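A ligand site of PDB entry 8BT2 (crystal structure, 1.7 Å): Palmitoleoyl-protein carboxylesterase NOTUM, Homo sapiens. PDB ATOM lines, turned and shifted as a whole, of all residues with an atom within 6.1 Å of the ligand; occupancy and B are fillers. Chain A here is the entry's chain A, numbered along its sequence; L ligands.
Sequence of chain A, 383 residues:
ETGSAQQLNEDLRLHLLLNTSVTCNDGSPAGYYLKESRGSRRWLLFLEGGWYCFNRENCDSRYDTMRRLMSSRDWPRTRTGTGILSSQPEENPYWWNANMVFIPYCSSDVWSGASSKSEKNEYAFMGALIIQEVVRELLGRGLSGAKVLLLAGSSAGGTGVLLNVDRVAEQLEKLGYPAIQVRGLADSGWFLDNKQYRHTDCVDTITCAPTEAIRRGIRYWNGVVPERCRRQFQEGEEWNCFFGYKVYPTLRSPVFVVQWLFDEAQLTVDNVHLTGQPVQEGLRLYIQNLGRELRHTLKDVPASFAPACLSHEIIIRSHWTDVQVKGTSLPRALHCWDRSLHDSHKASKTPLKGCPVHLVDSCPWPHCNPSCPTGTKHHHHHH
An oxygen (O1) of the ligand sits at hydrogen-bond distance from the side-chain hydroxyl (OG) of Ser 155. The backbone NH (N) of Ala 156 is in hydrogen-bond range of an oxygen (O1) of the ligand (3.3 Å).
A ring nitrogen (NE2) of His 312 is in hydrogen-bond range of the side-chain hydroxyl of Ser 155, at 3.1 Å. O of Gly 189 sits at hydrogen-bond distance from OG1 of Thr 159 (3.0 Å). OD1 of Asp 263 sits at hydrogen-bond distance from N of Ala 265, at 2.9 Å. The side-chain carboxylate (OD2) of Asp 263 lies within hydrogen-bond range of a ring nitrogen (ND1) of His 312.
CE2 of Trp 51 touches C1 of the ligand, 3.3 Å away. Tyr 52 touches the ligand. Thr 159 touches the ligand (OG1 to C8, 3.5 Å). Phe 191 touches the ligand (CB to F1, 3.1 Å). Pro 210 touches the ligand (CB to F3, 3.4 Å). Ile 214 touches the ligand. Phe 242 touches the ligand. Phe 243 touches the ligand. CB of Ala 265 touches C3 of the ligand, at 3.7 Å. Val 269 touches the ligand. NE2 of His 312 touches C1 of the ligand (3.9997 Å). Hydrophobic or aromatic side chains that line the ligand: Trp 51, Tyr 52, Ala 156, Phe 191, Pro 210, Ile 214, Phe 242, Phe 243, Ala 265 and Val 269. Of the 27 residues printed, 13 come within 4 Å of the ligand.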
ATOM      1  N   GLY A  49     -12.385   9.002  -3.094  1.00  0.00           N
ATOM      2  CA  GLY A  49     -11.153   9.696  -2.791  1.00  0.00           C
ATOM      3  C   GLY A  49      -9.936   8.905  -3.225  1.00  0.00           C
ATOM      4  O   GLY A  49     -10.018   7.894  -3.918  1.00  0.00           O
ATOM      5  N   GLY A  50      -8.763   9.403  -2.825  1.00  0.00           N
ATOM      6  CA  GLY A  50      -7.524   8.724  -3.138  1.00  0.00           C
ATOM      7  C   GLY A  50      -6.368   9.659  -3.439  1.00  0.00           C
ATOM      8  O   GLY A  50      -5.650   9.464  -4.421  1.00  0.00           O
ATOM      9  N   TRP A  51      -6.169  10.653  -2.577  1.00  0.00           N
ATOM     10  CA  TRP A  51      -5.048  11.605  -2.669  1.00  0.00           C
ATOM     11  C   TRP A  51      -5.126  12.328  -4.025  1.00  0.00           C
ATOM     12  O   TRP A  51      -6.228  12.715  -4.446  1.00  0.00           O
ATOM     13  CB  TRP A  51      -3.732  10.884  -2.418  1.00  0.00           C
ATOM     14  CG  TRP A  51      -3.490  10.524  -0.979  1.00  0.00           C
ATOM     15  CD1 TRP A  51      -3.740   9.324  -0.383  1.00  0.00           C
ATOM     16  CD2 TRP A  51      -2.929  11.370   0.026  1.00  0.00           C
ATOM     17  NE1 TRP A  51      -3.390   9.373   0.944  1.00  0.00           N
ATOM     18  CE2 TRP A  51      -2.881  10.616   1.216  1.00  0.00           C
ATOM     19  CE3 TRP A  51      -2.473  12.693   0.050  1.00  0.00           C
ATOM     20  CZ2 TRP A  51      -2.397  11.140   2.416  1.00  0.00           C
ATOM     21  CZ3 TRP A  51      -1.992  13.206   1.243  1.00  0.00           C
ATOM     22  CH2 TRP A  51      -1.952  12.434   2.408  1.00  0.00           C
ATOM     23  N   TYR A  52      -3.997  12.519  -4.705  1.00  0.00           N
ATOM     24  CA  TYR A  52      -3.870  13.343  -5.898  1.00  0.00           C
ATOM     25  C   TYR A  52      -2.414  13.234  -6.357  1.00  0.00           C
ATOM     26  O   TYR A  52      -1.581  12.621  -5.687  1.00  0.00           O
ATOM     27  CB  TYR A  52      -4.239  14.800  -5.622  1.00  0.00           C
ATOM     28  CG  TYR A  52      -3.688  15.324  -4.310  1.00  0.00           C
ATOM     29  CD1 TYR A  52      -2.349  15.676  -4.189  1.00  0.00           C
ATOM     30  CD2 TYR A  52      -4.499  15.446  -3.184  1.00  0.00           C
ATOM     31  CE1 TYR A  52      -1.842  16.147  -2.990  1.00  0.00           C
ATOM     32  CE2 TYR A  52      -3.995  15.904  -1.991  1.00  0.00           C
ATOM     33  CZ  TYR A  52      -2.672  16.258  -1.899  1.00  0.00           C
ATOM     34  OH  TYR A  52      -2.155  16.727  -0.701  1.00  0.00           O
ATOM     35  N   VAL A 110      -8.476  16.152  -7.120  1.00  0.00           N
ATOM     36  CA  VAL A 110      -9.370  16.532  -6.029  1.00  0.00           C
ATOM     37  C   VAL A 110     -10.690  16.976  -6.680  1.00  0.00           C
ATOM     38  O   VAL A 110     -11.401  17.850  -6.167  1.00  0.00           O
ATOM     39  CB  VAL A 110      -8.726  17.612  -5.128  1.00  0.00           C
ATOM     40  CG1 VAL A 110      -9.620  18.027  -3.962  1.00  0.00           C
ATOM     41  CG2 VAL A 110      -7.363  17.127  -4.627  1.00  0.00           C
ATOM     42  N   SER A 155     -12.716  11.833   1.724  1.00  0.00           N
ATOM     43  CA  SER A 155     -11.313  12.233   1.586  1.00  0.00           C
ATOM     44  C   SER A 155     -11.211  13.244   0.440  1.00  0.00           C
ATOM     45  O   SER A 155     -11.865  14.301   0.526  1.00  0.00           O
ATOM     46  CB  SER A 155     -10.452  10.974   1.444  1.00  0.00           C
ATOM     47  OG  SER A 155      -9.086  11.312   1.270  1.00  0.00           O
ATOM     48  N   ALA A 156     -10.435  12.980  -0.612  1.00  0.00           N
ATOM     49  CA  ALA A 156     -10.405  13.905  -1.745  1.00  0.00           C
ATOM     50  C   ALA A 156     -11.780  14.066  -2.370  1.00  0.00           C
ATOM     51  O   ALA A 156     -12.092  15.118  -2.934  1.00  0.00           O
ATOM     52  CB  ALA A 156      -9.392  13.415  -2.790  1.00  0.00           C
ATOM     53  N   GLY A 157     -12.618  13.025  -2.293  1.00  0.00           N
ATOM     54  CA  GLY A 157     -13.988  13.159  -2.739  1.00  0.00           C
ATOM     55  C   GLY A 157     -14.806  14.081  -1.845  1.00  0.00           C
ATOM     56  O   GLY A 157     -15.724  14.760  -2.330  1.00  0.00           O
ATOM     57  N   THR A 159     -13.551  16.798  -0.281  1.00  0.00           N
ATOM     58  CA  THR A 159     -13.188  18.119  -0.772  1.00  0.00           C
ATOM     59  C   THR A 159     -13.830  18.377  -2.128  1.00  0.00           C
ATOM     60  O   THR A 159     -14.237  19.504  -2.420  1.00  0.00           O
ATOM     61  CB  THR A 159     -11.662  18.245  -0.879  1.00  0.00           C
ATOM     62  OG1 THR A 159     -11.064  17.801   0.351  1.00  0.00           O
ATOM     63  CG2 THR A 159     -11.268  19.696  -1.127  1.00  0.00           C
ATOM     64  N   SER A 188     -14.482  13.722   5.526  1.00  0.00           N
ATOM     65  CA  SER A 188     -13.026  13.673   5.642  1.00  0.00           C
ATOM     66  C   SER A 188     -12.322  14.507   4.575  1.00  0.00           C
ATOM     67  O   SER A 188     -11.213  14.179   4.145  1.00  0.00           O
ATOM     68  CB  SER A 188     -12.523  12.220   5.600  1.00  0.00           C
ATOM     69  OG  SER A 188     -12.999  11.507   6.732  1.00  0.00           O
ATOM     70  N   GLY A 189     -12.948  15.607   4.154  1.00  0.00           N
ATOM     71  CA  GLY A 189     -12.348  16.501   3.182  1.00  0.00           C
ATOM     72  C   GLY A 189     -12.226  17.924   3.694  1.00  0.00           C
ATOM     73  O   GLY A 189     -12.105  18.871   2.908  1.00  0.00           O
ATOM     74  N   PHE A 191      -9.945  20.122   5.611  1.00  0.00           N
ATOM     75  CA  PHE A 191      -8.556  20.173   6.016  1.00  0.00           C
ATOM     76  C   PHE A 191      -8.147  21.583   6.425  1.00  0.00           C
ATOM     77  O   PHE A 191      -8.786  22.577   6.062  1.00  0.00           O
ATOM     78  CB  PHE A 191      -7.644  19.675   4.893  1.00  0.00           C
ATOM     79  CG  PHE A 191      -7.886  18.256   4.496  1.00  0.00           C
ATOM     80  CD1 PHE A 191      -7.422  17.211   5.277  1.00  0.00           C
ATOM     81  CD2 PHE A 191      -8.614  17.959   3.356  1.00  0.00           C
ATOM     82  CE1 PHE A 191      -7.659  15.900   4.923  1.00  0.00           C
ATOM     83  CE2 PHE A 191      -8.853  16.645   2.992  1.00  0.00           C
ATOM     84  CZ  PHE A 191      -8.376  15.620   3.774  1.00  0.00           C
ATOM     85  N   LEU A 192      -7.060  21.656   7.183  1.00  0.00           N
ATOM     86  CA  LEU A 192      -6.510  22.899   7.692  1.00  0.00           C
ATOM     87  C   LEU A 192      -5.188  23.193   7.016  1.00  0.00           C
ATOM     88  O   LEU A 192      -4.344  22.297   6.885  1.00  0.00           O
ATOM     89  CB  LEU A 192      -6.322  22.831   9.206  1.00  0.00           C
ATOM     90  CG  LEU A 192      -7.574  22.563  10.040  1.00  0.00           C
ATOM     91  CD1 LEU A 192      -7.215  22.605  11.507  1.00  0.00           C
ATOM     92  CD2 LEU A 192      -8.654  23.573   9.724  1.00  0.00           C
ATOM     93  N   ASP A 193      -4.997  24.433   6.595  1.00  0.00           N
ATOM     94  CA  ASP A 193      -3.704  24.881   6.062  1.00  0.00           C
ATOM     95  C   ASP A 193      -2.814  25.360   7.212  1.00  0.00           C
ATOM     96  O   ASP A 193      -2.339  26.499   7.255  1.00  0.00           O
ATOM     97  CB  ASP A 193      -3.906  25.952   4.999  1.00  0.00           C
ATOM     98  CG  ASP A 193      -4.796  27.088   5.468  1.00  0.00           C
ATOM     99  OD1 ASP A 193      -5.562  26.893   6.442  1.00  0.00           O
ATOM    100  OD2 ASP A 193      -4.728  28.173   4.869  1.00  0.00           O
ATOM    101  N   CYS A 208       3.897  16.543   1.555  1.00  0.00           N
ATOM    102  CA  CYS A 208       3.931  17.941   1.160  1.00  0.00           C
ATOM    103  C   CYS A 208       2.926  18.729   1.993  1.00  0.00           C
ATOM    104  O   CYS A 208       1.810  18.265   2.257  1.00  0.00           O
ATOM    105  CB  CYS A 208       3.604  18.080  -0.328  1.00  0.00           C
ATOM    106  SG  CYS A 208       3.521  19.776  -0.935  1.00  0.00           S
ATOM    107  N   ALA A 209       3.327  19.924   2.416  1.00  0.00           N
ATOM    108  CA  ALA A 209       2.454  20.764   3.208  1.00  0.00           C
ATOM    109  C   ALA A 209       1.159  21.060   2.434  1.00  0.00           C
ATOM    110  O   ALA A 209       1.180  21.143   1.206  1.00  0.00           O
ATOM    111  CB  ALA A 209       3.151  22.079   3.581  1.00  0.00           C
ATOM    112  N   PRO A 210       0.029  21.193   3.134  1.00  0.00           N
ATOM    113  CA  PRO A 210      -1.256  21.376   2.436  1.00  0.00           C
ATOM    114  C   PRO A 210      -1.274  22.531   1.449  1.00  0.00           C
ATOM    115  O   PRO A 210      -1.745  22.363   0.309  1.00  0.00           O
ATOM    116  CB  PRO A 210      -2.246  21.581   3.583  1.00  0.00           C
ATOM    117  CG  PRO A 210      -1.637  20.892   4.745  1.00  0.00           C
ATOM    118  CD  PRO A 210      -0.148  21.040   4.598  1.00  0.00           C
ATOM    119  N   THR A 211      -0.769  23.708   1.839  1.00  0.00           N
ATOM    120  CA  THR A 211      -0.836  24.867   0.951  1.00  0.00           C
ATOM    121  C   THR A 211      -0.017  24.658  -0.313  1.00  0.00           C
ATOM    122  O   THR A 211      -0.474  24.963  -1.419  1.00  0.00           O
ATOM    123  CB  THR A 211      -0.357  26.127   1.689  1.00  0.00           C
ATOM    124  OG1 THR A 211       1.060  26.062   1.874  1.00  0.00           O
ATOM    125  CG2 THR A 211      -1.036  26.249   3.039  1.00  0.00           C
ATOM    126  N   ALA A 213       1.005  21.853  -1.760  1.00  0.00           N
ATOM    127  CA  ALA A 213       0.477  20.808  -2.627  1.00  0.00           C
ATOM    128  C   ALA A 213      -0.652  21.342  -3.507  1.00  0.00           C
ATOM    129  O   ALA A 213      -0.686  21.078  -4.712  1.00  0.00           O
ATOM    130  CB  ALA A 213      -0.015  19.624  -1.778  1.00  0.00           C
ATOM    131  N   ILE A 214      -1.569  22.108  -2.918  1.00  0.00           N
ATOM    132  CA  ILE A 214      -2.708  22.609  -3.677  1.00  0.00           C
ATOM    133  C   ILE A 214      -2.285  23.735  -4.620  1.00  0.00           C
ATOM    134  O   ILE A 214      -2.778  23.826  -5.747  1.00  0.00           O
ATOM    135  CB  ILE A 214      -3.829  23.047  -2.717  1.00  0.00           C
ATOM    136  CG1 ILE A 214      -4.288  21.865  -1.855  1.00  0.00           C
ATOM    137  CG2 ILE A 214      -5.004  23.616  -3.499  1.00  0.00           C
ATOM    138  CD1 ILE A 214      -4.574  20.602  -2.654  1.00  0.00           C
ATOM    139  N   PHE A 242      -9.813  25.230  -1.743  1.00  0.00           N
ATOM    140  CA  PHE A 242      -9.741  23.807  -1.465  1.00  0.00           C
ATOM    141  C   PHE A 242      -9.863  23.500   0.021  1.00  0.00           C
ATOM    142  O   PHE A 242      -9.902  22.317   0.394  1.00  0.00           O
ATOM    143  CB  PHE A 242      -8.432  23.214  -1.985  1.00  0.00           C
ATOM    144  CG  PHE A 242      -8.419  22.981  -3.470  1.00  0.00           C
ATOM    145  CD1 PHE A 242      -8.498  24.050  -4.349  1.00  0.00           C
ATOM    146  CD2 PHE A 242      -8.292  21.700  -3.973  1.00  0.00           C
ATOM    147  CE1 PHE A 242      -8.477  23.835  -5.713  1.00  0.00           C
ATOM    148  CE2 PHE A 242      -8.271  21.486  -5.337  1.00  0.00           C
ATOM    149  CZ  PHE A 242      -8.359  22.556  -6.214  1.00  0.00           C
ATOM    150  N   PHE A 243      -9.921  24.512   0.880  1.00  0.00           N
ATOM    151  CA  PHE A 243      -9.912  24.327   2.315  1.00  0.00           C
ATOM    152  C   PHE A 243     -11.296  24.649   2.862  1.00  0.00           C
ATOM    153  O   PHE A 243     -11.796  25.764   2.674  1.00  0.00           O
ATOM    154  CB  PHE A 243      -8.828  25.186   2.963  1.00  0.00           C
ATOM    155  CG  PHE A 243      -7.432  24.685   2.683  1.00  0.00           C
ATOM    156  CD1 PHE A 243      -6.852  23.739   3.500  1.00  0.00           C
ATOM    157  CD2 PHE A 243      -6.747  25.113   1.562  1.00  0.00           C
ATOM    158  CE1 PHE A 243      -5.584  23.254   3.239  1.00  0.00           C
ATOM    159  CE2 PHE A 243      -5.481  24.635   1.288  1.00  0.00           C
ATOM    160  CZ  PHE A 243      -4.893  23.706   2.130  1.00  0.00           C
ATOM    161  N   ASP A 263      -7.831  13.779  12.049  1.00  0.00           N
ATOM    162  CA  ASP A 263      -7.850  13.037  10.804  1.00  0.00           C
ATOM    163  C   ASP A 263      -6.446  12.564  10.449  1.00  0.00           C
ATOM    164  O   ASP A 263      -5.474  13.324  10.509  1.00  0.00           O
ATOM    165  CB  ASP A 263      -8.424  13.905   9.686  1.00  0.00           C
ATOM    166  CG  ASP A 263      -8.499  13.174   8.366  1.00  0.00           C
ATOM    167  OD1 ASP A 263      -7.515  13.210   7.599  1.00  0.00           O
ATOM    168  OD2 ASP A 263      -9.550  12.560   8.087  1.00  0.00           O
ATOM    169  N   ALA A 265      -5.122  11.661   7.561  1.00  0.00           N
ATOM    170  CA  ALA A 265      -4.534  12.297   6.380  1.00  0.00           C
ATOM    171  C   ALA A 265      -4.051  13.706   6.704  1.00  0.00           C
ATOM    172  O   ALA A 265      -3.017  14.144   6.178  1.00  0.00           O
ATOM    173  CB  ALA A 265      -5.539  12.311   5.227  1.00  0.00           C
ATOM    174  N   GLN A 266      -4.784  14.427   7.550  1.00  0.00           N
ATOM    175  CA  GLN A 266      -4.326  15.728   8.022  1.00  0.00           C
ATOM    176  C   GLN A 266      -3.002  15.600   8.769  1.00  0.00           C
ATOM    177  O   GLN A 266      -2.077  16.380   8.556  1.00  0.00           O
ATOM    178  CB  GLN A 266      -5.392  16.363   8.918  1.00  0.00           C
ATOM    179  CG  GLN A 266      -4.958  17.668   9.557  1.00  0.00           C
ATOM    180  CD  GLN A 266      -5.077  18.845   8.613  1.00  0.00           C
ATOM    181  OE1 GLN A 266      -6.127  19.073   8.010  1.00  0.00           O
ATOM    182  NE2 GLN A 266      -3.987  19.600   8.460  1.00  0.00           N
ATOM    183  N   VAL A 269      -0.013  14.883   6.183  1.00  0.00           N
ATOM    184  CA  VAL A 269       0.541  16.061   5.524  1.00  0.00           C
ATOM    185  C   VAL A 269       1.161  17.020   6.533  1.00  0.00           C
ATOM    186  O   VAL A 269       1.967  17.881   6.153  1.00  0.00           O
ATOM    187  CB  VAL A 269      -0.542  16.784   4.682  1.00  0.00           C
ATOM    188  CG1 VAL A 269      -1.013  15.899   3.546  1.00  0.00           C
ATOM    189  CG2 VAL A 269      -1.703  17.218   5.556  1.00  0.00           C
ATOM    190  N   HIS A 312      -9.721   8.045   9.400  1.00  0.00           N
ATOM    191  CA  HIS A 312      -9.834   8.680   8.091  1.00  0.00           C
ATOM    192  C   HIS A 312     -10.975   8.021   7.332  1.00  0.00           C
ATOM    193  O   HIS A 312     -10.999   6.794   7.187  1.00  0.00           O
ATOM    194  CB  HIS A 312      -8.524   8.550   7.310  1.00  0.00           C
ATOM    195  CG  HIS A 312      -8.511   9.318   6.014  1.00  0.00           C
ATOM    196  ND1 HIS A 312      -8.885  10.637   5.934  1.00  0.00           N
ATOM    197  CD2 HIS A 312      -8.168   8.938   4.767  1.00  0.00           C
ATOM    198  CE1 HIS A 312      -8.780  11.043   4.681  1.00  0.00           C
ATOM    199  NE2 HIS A 312      -8.343  10.033   3.948  1.00  0.00           N
HETATM  200  C1  LIG L   1      -5.926  11.943   1.397  1.00  0.00           C
HETATM  201  C2  LIG L   1      -6.452  13.237   0.783  1.00  0.00           C
HETATM  202  C3  LIG L   1      -5.062  14.665   2.404  1.00  0.00           C
HETATM  203  C4  LIG L   1      -4.560  16.078   2.291  1.00  0.00           C
HETATM  204  C5  LIG L   1      -5.583  16.821   1.427  1.00  0.00           C
HETATM  205  C6  LIG L   1      -6.410  15.857   0.841  1.00  0.00           C
HETATM  206  C7  LIG L   1      -7.462  16.246  -0.015  1.00  0.00           C
HETATM  207  C8  LIG L   1      -7.677  17.587  -0.284  1.00  0.00           C
HETATM  208  C9  LIG L   1      -6.842  18.556   0.288  1.00  0.00           C
HETATM  209  C10 LIG L   1      -5.796  18.190   1.149  1.00  0.00           C
HETATM  210  C11 LIG L   1      -4.936  19.318   1.730  1.00  0.00           C
HETATM  211  F1  LIG L   1      -5.674  20.056   2.594  1.00  0.00           F
HETATM  212  F2  LIG L   1      -4.536  20.126   0.708  1.00  0.00           F
HETATM  213  F3  LIG L   1      -3.817  18.865   2.372  1.00  0.00           F
HETATM  214  N1  LIG L   1      -5.988  14.502   1.307  1.00  0.00           N
HETATM  215  O1  LIG L   1      -7.216  13.197  -0.126  1.00  0.00           O
HETATM  216 CL1  LIG L   1      -7.137  20.273  -0.075  1.00  0.00          CL
